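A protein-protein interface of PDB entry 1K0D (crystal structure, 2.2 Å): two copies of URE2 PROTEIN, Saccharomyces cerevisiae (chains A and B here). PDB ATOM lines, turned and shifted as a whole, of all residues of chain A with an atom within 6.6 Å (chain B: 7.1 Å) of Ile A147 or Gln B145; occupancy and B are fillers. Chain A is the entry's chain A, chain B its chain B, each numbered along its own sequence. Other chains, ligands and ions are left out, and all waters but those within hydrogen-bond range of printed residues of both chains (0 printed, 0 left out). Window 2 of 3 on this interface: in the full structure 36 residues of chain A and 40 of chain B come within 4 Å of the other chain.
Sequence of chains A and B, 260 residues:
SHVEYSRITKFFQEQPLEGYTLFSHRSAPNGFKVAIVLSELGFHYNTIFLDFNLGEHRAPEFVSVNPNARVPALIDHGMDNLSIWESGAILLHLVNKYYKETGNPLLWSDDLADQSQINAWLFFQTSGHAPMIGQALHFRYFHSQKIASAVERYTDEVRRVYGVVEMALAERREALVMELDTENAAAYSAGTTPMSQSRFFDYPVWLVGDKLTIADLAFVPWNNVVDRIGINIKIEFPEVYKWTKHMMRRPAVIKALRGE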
ATOM      1  N   PHE A 139      11.285 -27.203  -9.763  1.00  0.00           N
ATOM      2  CA  PHE A 139      10.556 -27.415 -11.012  1.00  0.00           C
ATOM      3  C   PHE A 139      11.474 -27.850 -12.136  1.00  0.00           C
ATOM      4  O   PHE A 139      11.034 -28.411 -13.137  1.00  0.00           O
ATOM      5  CB  PHE A 139       9.794 -26.149 -11.417  1.00  0.00           C
ATOM      6  CG  PHE A 139       8.576 -25.896 -10.579  1.00  0.00           C
ATOM      7  CD1 PHE A 139       8.589 -24.939  -9.573  1.00  0.00           C
ATOM      8  CD2 PHE A 139       7.426 -26.659 -10.764  1.00  0.00           C
ATOM      9  CE1 PHE A 139       7.475 -24.744  -8.755  1.00  0.00           C
ATOM     10  CE2 PHE A 139       6.310 -26.473  -9.953  1.00  0.00           C
ATOM     11  CZ  PHE A 139       6.336 -25.511  -8.944  1.00  0.00           C
ATOM     12  N   ARG A 140      12.759 -27.591 -11.960  1.00  0.00           N
ATOM     13  CA  ARG A 140      13.746 -27.957 -12.954  1.00  0.00           C
ATOM     14  C   ARG A 140      14.173 -29.416 -12.796  1.00  0.00           C
ATOM     15  O   ARG A 140      14.341 -30.122 -13.781  1.00  0.00           O
ATOM     16  CB  ARG A 140      14.964 -27.049 -12.820  1.00  0.00           C
ATOM     17  CG  ARG A 140      16.142 -27.442 -13.672  1.00  0.00           C
ATOM     18  CD  ARG A 140      16.235 -26.601 -14.920  1.00  0.00           C
ATOM     19  NE  ARG A 140      17.564 -26.697 -15.512  1.00  0.00           N
ATOM     20  CZ  ARG A 140      17.943 -26.065 -16.617  1.00  0.00           C
ATOM     21  NH1 ARG A 140      19.181 -26.220 -17.072  1.00  0.00           N
ATOM     22  NH2 ARG A 140      17.088 -25.282 -17.266  1.00  0.00           N
ATOM     23  N   HIS A 143      10.160 -31.793  -9.682  1.00  0.00           N
ATOM     24  CA  HIS A 143       8.709 -31.752  -9.654  1.00  0.00           C
ATOM     25  C   HIS A 143       8.141 -32.998 -10.322  1.00  0.00           C
ATOM     26  O   HIS A 143       8.783 -33.596 -11.184  1.00  0.00           O
ATOM     27  CB  HIS A 143       8.170 -30.508 -10.348  1.00  0.00           C
ATOM     28  CG  HIS A 143       6.760 -30.184  -9.965  1.00  0.00           C
ATOM     29  ND1 HIS A 143       5.754 -30.017 -10.891  1.00  0.00           N
ATOM     30  CD2 HIS A 143       6.190 -29.998  -8.751  1.00  0.00           C
ATOM     31  CE1 HIS A 143       4.625 -29.740 -10.265  1.00  0.00           C
ATOM     32  NE2 HIS A 143       4.863 -29.722  -8.966  1.00  0.00           N
ATOM     33  N   GLN A 145       5.971 -33.148 -12.402  1.00  0.00           N
ATOM     34  CA  GLN A 145       5.649 -32.855 -13.793  1.00  0.00           C
ATOM     35  C   GLN A 145       6.613 -31.796 -14.317  1.00  0.00           C
ATOM     36  O   GLN A 145       7.056 -30.930 -13.566  1.00  0.00           O
ATOM     37  CB  GLN A 145       4.202 -32.352 -13.888  1.00  0.00           C
ATOM     38  CG  GLN A 145       3.672 -32.194 -15.302  1.00  0.00           C
ATOM     39  CD  GLN A 145       2.212 -31.755 -15.335  1.00  0.00           C
ATOM     40  OE1 GLN A 145       1.353 -32.378 -14.711  1.00  0.00           O
ATOM     41  NE2 GLN A 145       1.929 -30.684 -16.070  1.00  0.00           N
ATOM     42  N   LYS A 146       6.933 -31.871 -15.604  1.00  0.00           N
ATOM     43  CA  LYS A 146       7.849 -30.921 -16.225  1.00  0.00           C
ATOM     44  C   LYS A 146       7.068 -29.761 -16.820  1.00  0.00           C
ATOM     45  O   LYS A 146       6.290 -29.940 -17.759  1.00  0.00           O
ATOM     46  CB  LYS A 146       8.677 -31.626 -17.305  1.00  0.00           C
ATOM     47  CG  LYS A 146       9.614 -30.722 -18.085  1.00  0.00           C
ATOM     48  CD  LYS A 146      10.947 -31.416 -18.371  1.00  0.00           C
ATOM     49  CE  LYS A 146      10.754 -32.787 -19.010  1.00  0.00           C
ATOM     50  NZ  LYS A 146      12.028 -33.573 -19.031  1.00  0.00           N
ATOM     51  N   ILE A 147       7.282 -28.569 -16.272  1.00  0.00           N
ATOM     52  CA  ILE A 147       6.577 -27.383 -16.729  1.00  0.00           C
ATOM     53  C   ILE A 147       7.532 -26.213 -16.920  1.00  0.00           C
ATOM     54  O   ILE A 147       8.009 -25.615 -15.951  1.00  0.00           O
ATOM     55  CB  ILE A 147       5.498 -26.983 -15.718  1.00  0.00           C
ATOM     56  CG1 ILE A 147       4.783 -28.238 -15.209  1.00  0.00           C
ATOM     57  CG2 ILE A 147       4.501 -26.052 -16.380  1.00  0.00           C
ATOM     58  CD1 ILE A 147       4.333 -28.141 -13.784  1.00  0.00           C
ATOM     59  N   ALA A 148       7.787 -25.880 -18.179  1.00  0.00           N
ATOM     60  CA  ALA A 148       8.701 -24.810 -18.521  1.00  0.00           C
ATOM     61  C   ALA A 148       8.348 -23.455 -17.920  1.00  0.00           C
ATOM     62  O   ALA A 148       9.227 -22.745 -17.436  1.00  0.00           O
ATOM     63  CB  ALA A 148       8.813 -24.697 -20.039  1.00  0.00           C
ATOM     64  N   SER A 149       7.069 -23.091 -17.945  1.00  0.00           N
ATOM     65  CA  SER A 149       6.660 -21.801 -17.407  1.00  0.00           C
ATOM     66  C   SER A 149       6.976 -21.653 -15.915  1.00  0.00           C
ATOM     67  O   SER A 149       7.214 -20.547 -15.443  1.00  0.00           O
ATOM     68  CB  SER A 149       5.167 -21.565 -17.649  1.00  0.00           C
ATOM     69  OG  SER A 149       4.385 -22.466 -16.903  1.00  0.00           O
ATOM     70  N   ALA A 150       6.972 -22.757 -15.178  1.00  0.00           N
ATOM     71  CA  ALA A 150       7.279 -22.702 -13.752  1.00  0.00           C
ATOM     72  C   ALA A 150       8.783 -22.470 -13.605  1.00  0.00           C
ATOM     73  O   ALA A 150       9.219 -21.639 -12.804  1.00  0.00           O
ATOM     74  CB  ALA A 150       6.871 -24.005 -13.063  1.00  0.00           C
ATOM     75  N   VAL A 151       9.572 -23.198 -14.391  1.00  0.00           N
ATOM     76  CA  VAL A 151      11.027 -23.053 -14.359  1.00  0.00           C
ATOM     77  C   VAL A 151      11.425 -21.625 -14.739  1.00  0.00           C
ATOM     78  O   VAL A 151      12.209 -20.984 -14.036  1.00  0.00           O
ATOM     79  CB  VAL A 151      11.716 -24.047 -15.338  1.00  0.00           C
ATOM     80  CG1 VAL A 151      13.214 -23.774 -15.404  1.00  0.00           C
ATOM     81  CG2 VAL A 151      11.478 -25.476 -14.886  1.00  0.00           C
ATOM     82  N   GLU A 152      10.873 -21.126 -15.842  1.00  0.00           N
ATOM     83  CA  GLU A 152      11.189 -19.782 -16.322  1.00  0.00           C
ATOM     84  C   GLU A 152      10.849 -18.717 -15.288  1.00  0.00           C
ATOM     85  O   GLU A 152      11.632 -17.790 -15.067  1.00  0.00           O
ATOM     86  CB  GLU A 152      10.438 -19.471 -17.626  1.00  0.00           C
ATOM     87  CG  GLU A 152      10.887 -18.167 -18.286  1.00  0.00           C
ATOM     88  CD  GLU A 152      10.000 -17.732 -19.452  1.00  0.00           C
ATOM     89  OE1 GLU A 152      10.438 -16.856 -20.235  1.00  0.00           O
ATOM     90  OE2 GLU A 152       8.865 -18.249 -19.579  1.00  0.00           O
ATOM     91  N   HIS B 138      -0.163 -16.994  -6.560  1.00  0.00           N
ATOM     92  CA  HIS B 138       0.241 -16.860  -7.957  1.00  0.00           C
ATOM     93  C   HIS B 138      -0.277 -17.983  -8.860  1.00  0.00           C
ATOM     94  O   HIS B 138      -0.916 -17.717  -9.875  1.00  0.00           O
ATOM     95  CB  HIS B 138       1.763 -16.797  -8.091  1.00  0.00           C
ATOM     96  CG  HIS B 138       2.226 -16.702  -9.511  1.00  0.00           C
ATOM     97  ND1 HIS B 138       2.113 -15.547 -10.252  1.00  0.00           N
ATOM     98  CD2 HIS B 138       2.709 -17.644 -10.357  1.00  0.00           C
ATOM     99  CE1 HIS B 138       2.503 -15.778 -11.494  1.00  0.00           C
ATOM    100  NE2 HIS B 138       2.870 -17.045 -11.584  1.00  0.00           N
ATOM    101  N   PHE B 139       0.000 -19.233  -8.504  1.00  0.00           N
ATOM    102  CA  PHE B 139      -0.444 -20.346  -9.337  1.00  0.00           C
ATOM    103  C   PHE B 139      -1.946 -20.578  -9.306  1.00  0.00           C
ATOM    104  O   PHE B 139      -2.519 -21.112 -10.252  1.00  0.00           O
ATOM    105  CB  PHE B 139       0.297 -21.631  -8.956  1.00  0.00           C
ATOM    106  CG  PHE B 139       1.739 -21.630  -9.371  1.00  0.00           C
ATOM    107  CD1 PHE B 139       2.752 -21.407  -8.439  1.00  0.00           C
ATOM    108  CD2 PHE B 139       2.083 -21.796 -10.712  1.00  0.00           C
ATOM    109  CE1 PHE B 139       4.090 -21.345  -8.840  1.00  0.00           C
ATOM    110  CE2 PHE B 139       3.411 -21.738 -11.120  1.00  0.00           C
ATOM    111  CZ  PHE B 139       4.418 -21.510 -10.180  1.00  0.00           C
ATOM    112  N   PHE B 142      -2.840 -16.142 -10.874  1.00  0.00           N
ATOM    113  CA  PHE B 142      -2.173 -15.331 -11.885  1.00  0.00           C
ATOM    114  C   PHE B 142      -1.180 -15.942 -12.860  1.00  0.00           C
ATOM    115  O   PHE B 142      -0.590 -15.214 -13.660  1.00  0.00           O
ATOM    116  CB  PHE B 142      -1.490 -14.146 -11.188  1.00  0.00           C
ATOM    117  CG  PHE B 142      -2.350 -13.467 -10.159  1.00  0.00           C
ATOM    118  CD1 PHE B 142      -2.180 -13.737  -8.803  1.00  0.00           C
ATOM    119  CD2 PHE B 142      -3.341 -12.563 -10.543  1.00  0.00           C
ATOM    120  CE1 PHE B 142      -2.990 -13.116  -7.836  1.00  0.00           C
ATOM    121  CE2 PHE B 142      -4.159 -11.934  -9.586  1.00  0.00           C
ATOM    122  CZ  PHE B 142      -3.980 -12.212  -8.230  1.00  0.00           C
ATOM    123  N   HIS B 143      -0.982 -17.253 -12.827  1.00  0.00           N
ATOM    124  CA  HIS B 143      -0.013 -17.836 -13.740  1.00  0.00           C
ATOM    125  C   HIS B 143      -0.536 -17.912 -15.178  1.00  0.00           C
ATOM    126  O   HIS B 143      -1.748 -17.956 -15.411  1.00  0.00           O
ATOM    127  CB  HIS B 143       0.406 -19.219 -13.253  1.00  0.00           C
ATOM    128  CG  HIS B 143       1.712 -19.681 -13.817  1.00  0.00           C
ATOM    129  ND1 HIS B 143       1.840 -20.844 -14.547  1.00  0.00           N
ATOM    130  CD2 HIS B 143       2.944 -19.122 -13.777  1.00  0.00           C
ATOM    131  CE1 HIS B 143       3.096 -20.981 -14.934  1.00  0.00           C
ATOM    132  NE2 HIS B 143       3.786 -19.950 -14.480  1.00  0.00           N
ATOM    133  N   SER B 144       0.391 -17.928 -16.134  1.00  0.00           N
ATOM    134  CA  SER B 144       0.054 -17.974 -17.554  1.00  0.00           C
ATOM    135  C   SER B 144      -0.768 -19.207 -17.924  1.00  0.00           C
ATOM    136  O   SER B 144      -1.395 -19.245 -18.979  1.00  0.00           O
ATOM    137  CB  SER B 144       1.329 -17.926 -18.403  1.00  0.00           C
ATOM    138  OG  SER B 144       2.126 -19.081 -18.207  1.00  0.00           O
ATOM    139  N   GLN B 145      -0.762 -20.214 -17.058  1.00  0.00           N
ATOM    140  CA  GLN B 145      -1.534 -21.422 -17.299  1.00  0.00           C
ATOM    141  C   GLN B 145      -1.811 -22.105 -15.966  1.00  0.00           C
ATOM    142  O   GLN B 145      -1.090 -21.897 -14.992  1.00  0.00           O
ATOM    143  CB  GLN B 145      -0.780 -22.366 -18.248  1.00  0.00           C
ATOM    144  CG  GLN B 145       0.459 -23.045 -17.659  1.00  0.00           C
ATOM    145  CD  GLN B 145       1.298 -23.751 -18.727  1.00  0.00           C
ATOM    146  OE1 GLN B 145       0.765 -24.423 -19.607  1.00  0.00           O
ATOM    147  NE2 GLN B 145       2.611 -23.606 -18.640  1.00  0.00           N
ATOM    148  N   LYS B 146      -2.870 -22.903 -15.919  1.00  0.00           N
ATOM    149  CA  LYS B 146      -3.236 -23.606 -14.699  1.00  0.00           C
ATOM    150  C   LYS B 146      -2.321 -24.801 -14.459  1.00  0.00           C
ATOM    151  O   LYS B 146      -2.110 -25.612 -15.355  1.00  0.00           O
ATOM    152  CB  LYS B 146      -4.695 -24.069 -14.791  1.00  0.00           C
ATOM    153  CG  LYS B 146      -5.033 -25.292 -13.954  1.00  0.00           C
ATOM    154  CD  LYS B 146      -6.484 -25.711 -14.169  1.00  0.00           C
ATOM    155  CE  LYS B 146      -6.764 -27.116 -13.640  1.00  0.00           C
ATOM    156  NZ  LYS B 146      -6.053 -28.172 -14.429  1.00  0.00           N
ATOM    157  N   ILE B 147      -1.779 -24.895 -13.246  1.00  0.00           N
ATOM    158  CA  ILE B 147      -0.892 -25.996 -12.871  1.00  0.00           C
ATOM    159  C   ILE B 147      -1.299 -26.533 -11.501  1.00  0.00           C
ATOM    160  O   ILE B 147      -0.744 -26.130 -10.473  1.00  0.00           O
ATOM    161  CB  ILE B 147       0.581 -25.538 -12.797  1.00  0.00           C
ATOM    162  CG1 ILE B 147       0.985 -24.858 -14.103  1.00  0.00           C
ATOM    163  CG2 ILE B 147       1.488 -26.740 -12.539  1.00  0.00           C
ATOM    164  CD1 ILE B 147       2.425 -24.381 -14.115  1.00  0.00           C
ATOM    165  N   ALA B 148      -2.265 -27.446 -11.493  1.00  0.00           N
ATOM    166  CA  ALA B 148      -2.764 -28.036 -10.253  1.00  0.00           C
ATOM    167  C   ALA B 148      -1.667 -28.531  -9.312  1.00  0.00           C
ATOM    168  O   ALA B 148      -1.775 -28.379  -8.092  1.00  0.00           O
ATOM    169  CB  ALA B 148      -3.723 -29.187 -10.570  1.00  0.00           C
ATOM    170  N   SER B 149      -0.621 -29.140  -9.867  1.00  0.00           N
ATOM    171  CA  SER B 149       0.456 -29.652  -9.030  1.00  0.00           C
ATOM    172  C   SER B 149       1.190 -28.518  -8.321  1.00  0.00           C
ATOM    173  O   SER B 149       1.671 -28.692  -7.205  1.00  0.00           O
ATOM    174  CB  SER B 149       1.438 -30.484  -9.861  1.00  0.00           C
ATOM    175  OG  SER B 149       1.947 -29.749 -10.959  1.00  0.00           O
ATOM    176  N   ALA B 150       1.266 -27.357  -8.964  1.00  0.00           N
ATOM    177  CA  ALA B 150       1.934 -26.206  -8.365  1.00  0.00           C
ATOM    178  C   ALA B 150       1.074 -25.653  -7.227  1.00  0.00           C
ATOM    179  O   ALA B 150       1.582 -25.334  -6.152  1.00  0.00           O
ATOM    180  CB  ALA B 150       2.172 -25.132  -9.417  1.00  0.00           C
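The side-chain amide nitrogen (NE2) of Gln B145 sits at hydrogen-bond distance from the side-chain hydroxyl (OG) of Ser A149, at 2.7 Å.
The backbone carbonyl oxygen of Gln B145 is in hydrogen-bond range of a ring nitrogen (ND1) of His B143 (3.1 Å).
A ring nitrogen (ND1) of His A143 lies within hydrogen-bond range of the backbone carbonyl oxygen of Gln A145, at 3.1 Å.
The backbone carbonyl oxygen (O) of His B138 is in hydrogen-bond range of the backbone NH (N) of His B143 (3.0 Å).
Ser B149 touches His A143 (OG to CE1, 2.8 Å).
NE2 of Gln B145 touches CG2 of Ile A147 (3.8 Å).
Ile A147 touches Ile B147 (CD1 to CG2, 3.4 Å).
His B143 touches Ser A149.
OG of Ser B144 touches CB of Ser A149, at 3.97 Å.
Ile B147 touches Ser A149 (CD1 to OG, 3.9 Å).
Printed residues of chain B within 4 Å of His A143: Ser B149 (2.8 Å).
Gln A145 touches none of the printed residues of chain B.
Ile A147 touches just these residues of chain B: Gln B145 (3.8 Å) and Ile B147 (3.4 Å).
Printed residues of chain B within 4 Å of Ser A149: His B143 (2.8 Å), Ser B144 (3.97 Å), Gln B145 (2.7 Å) and Ile B147 (3.9 Å).
His B138 touches none of the printed residues of chain A.
Of the printed residues of chain A, His B143 touches Ser A149.
Of the printed residues of chain A, Ser B144 touches Ser A149.
Of chain A, only Ile A147 (3.8 Å) and Ser A149 (2.7 Å) come within 4 Å of Gln B145.
Printed residues of chain A within 4 Å of Ser B149: His A143 (2.8 Å).
The nearest residue of chain B that does not touch Ile A147 is Ser B149 (4.03 Å).
The nearest printed residue of chain A that does not touch Ser B144 is Ala A150 (6.8 Å).
Of the 11 printed residues of chain B, 5 touch a printed residue of chain A.
Hydrophobic or aromatic side chains of chain B that line the printed part of chain A: His B143 and Ile B147.
Hydrophobic or aromatic side chains of chain A within 4 Å of the printed part of chain B: His A143 and Ile A147.
Among the printed residues, 7 pairs touch across the chains.
Among the printed residues, no Asp or Glu carboxylate lies within 4 Å of a Lys or Arg side-chain nitrogen of the other chain.
His A143 touches Ser B149, and with the chains exchanged Ser A149 touches His B143.
Ile A147 touches Gln B145, but with the chains exchanged Gln A145 does not touch Ile B147 (5.3 Å).
Ser A149 touches Gln B145, but with the chains exchanged Gln A145 does not touch Ser B149 (4.5 Å).
Ser A149 touches Ile B147, but with the chains exchanged Ile A147 does not touch Ser B149 (4.03 Å).
8 positions are printed for both chains.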
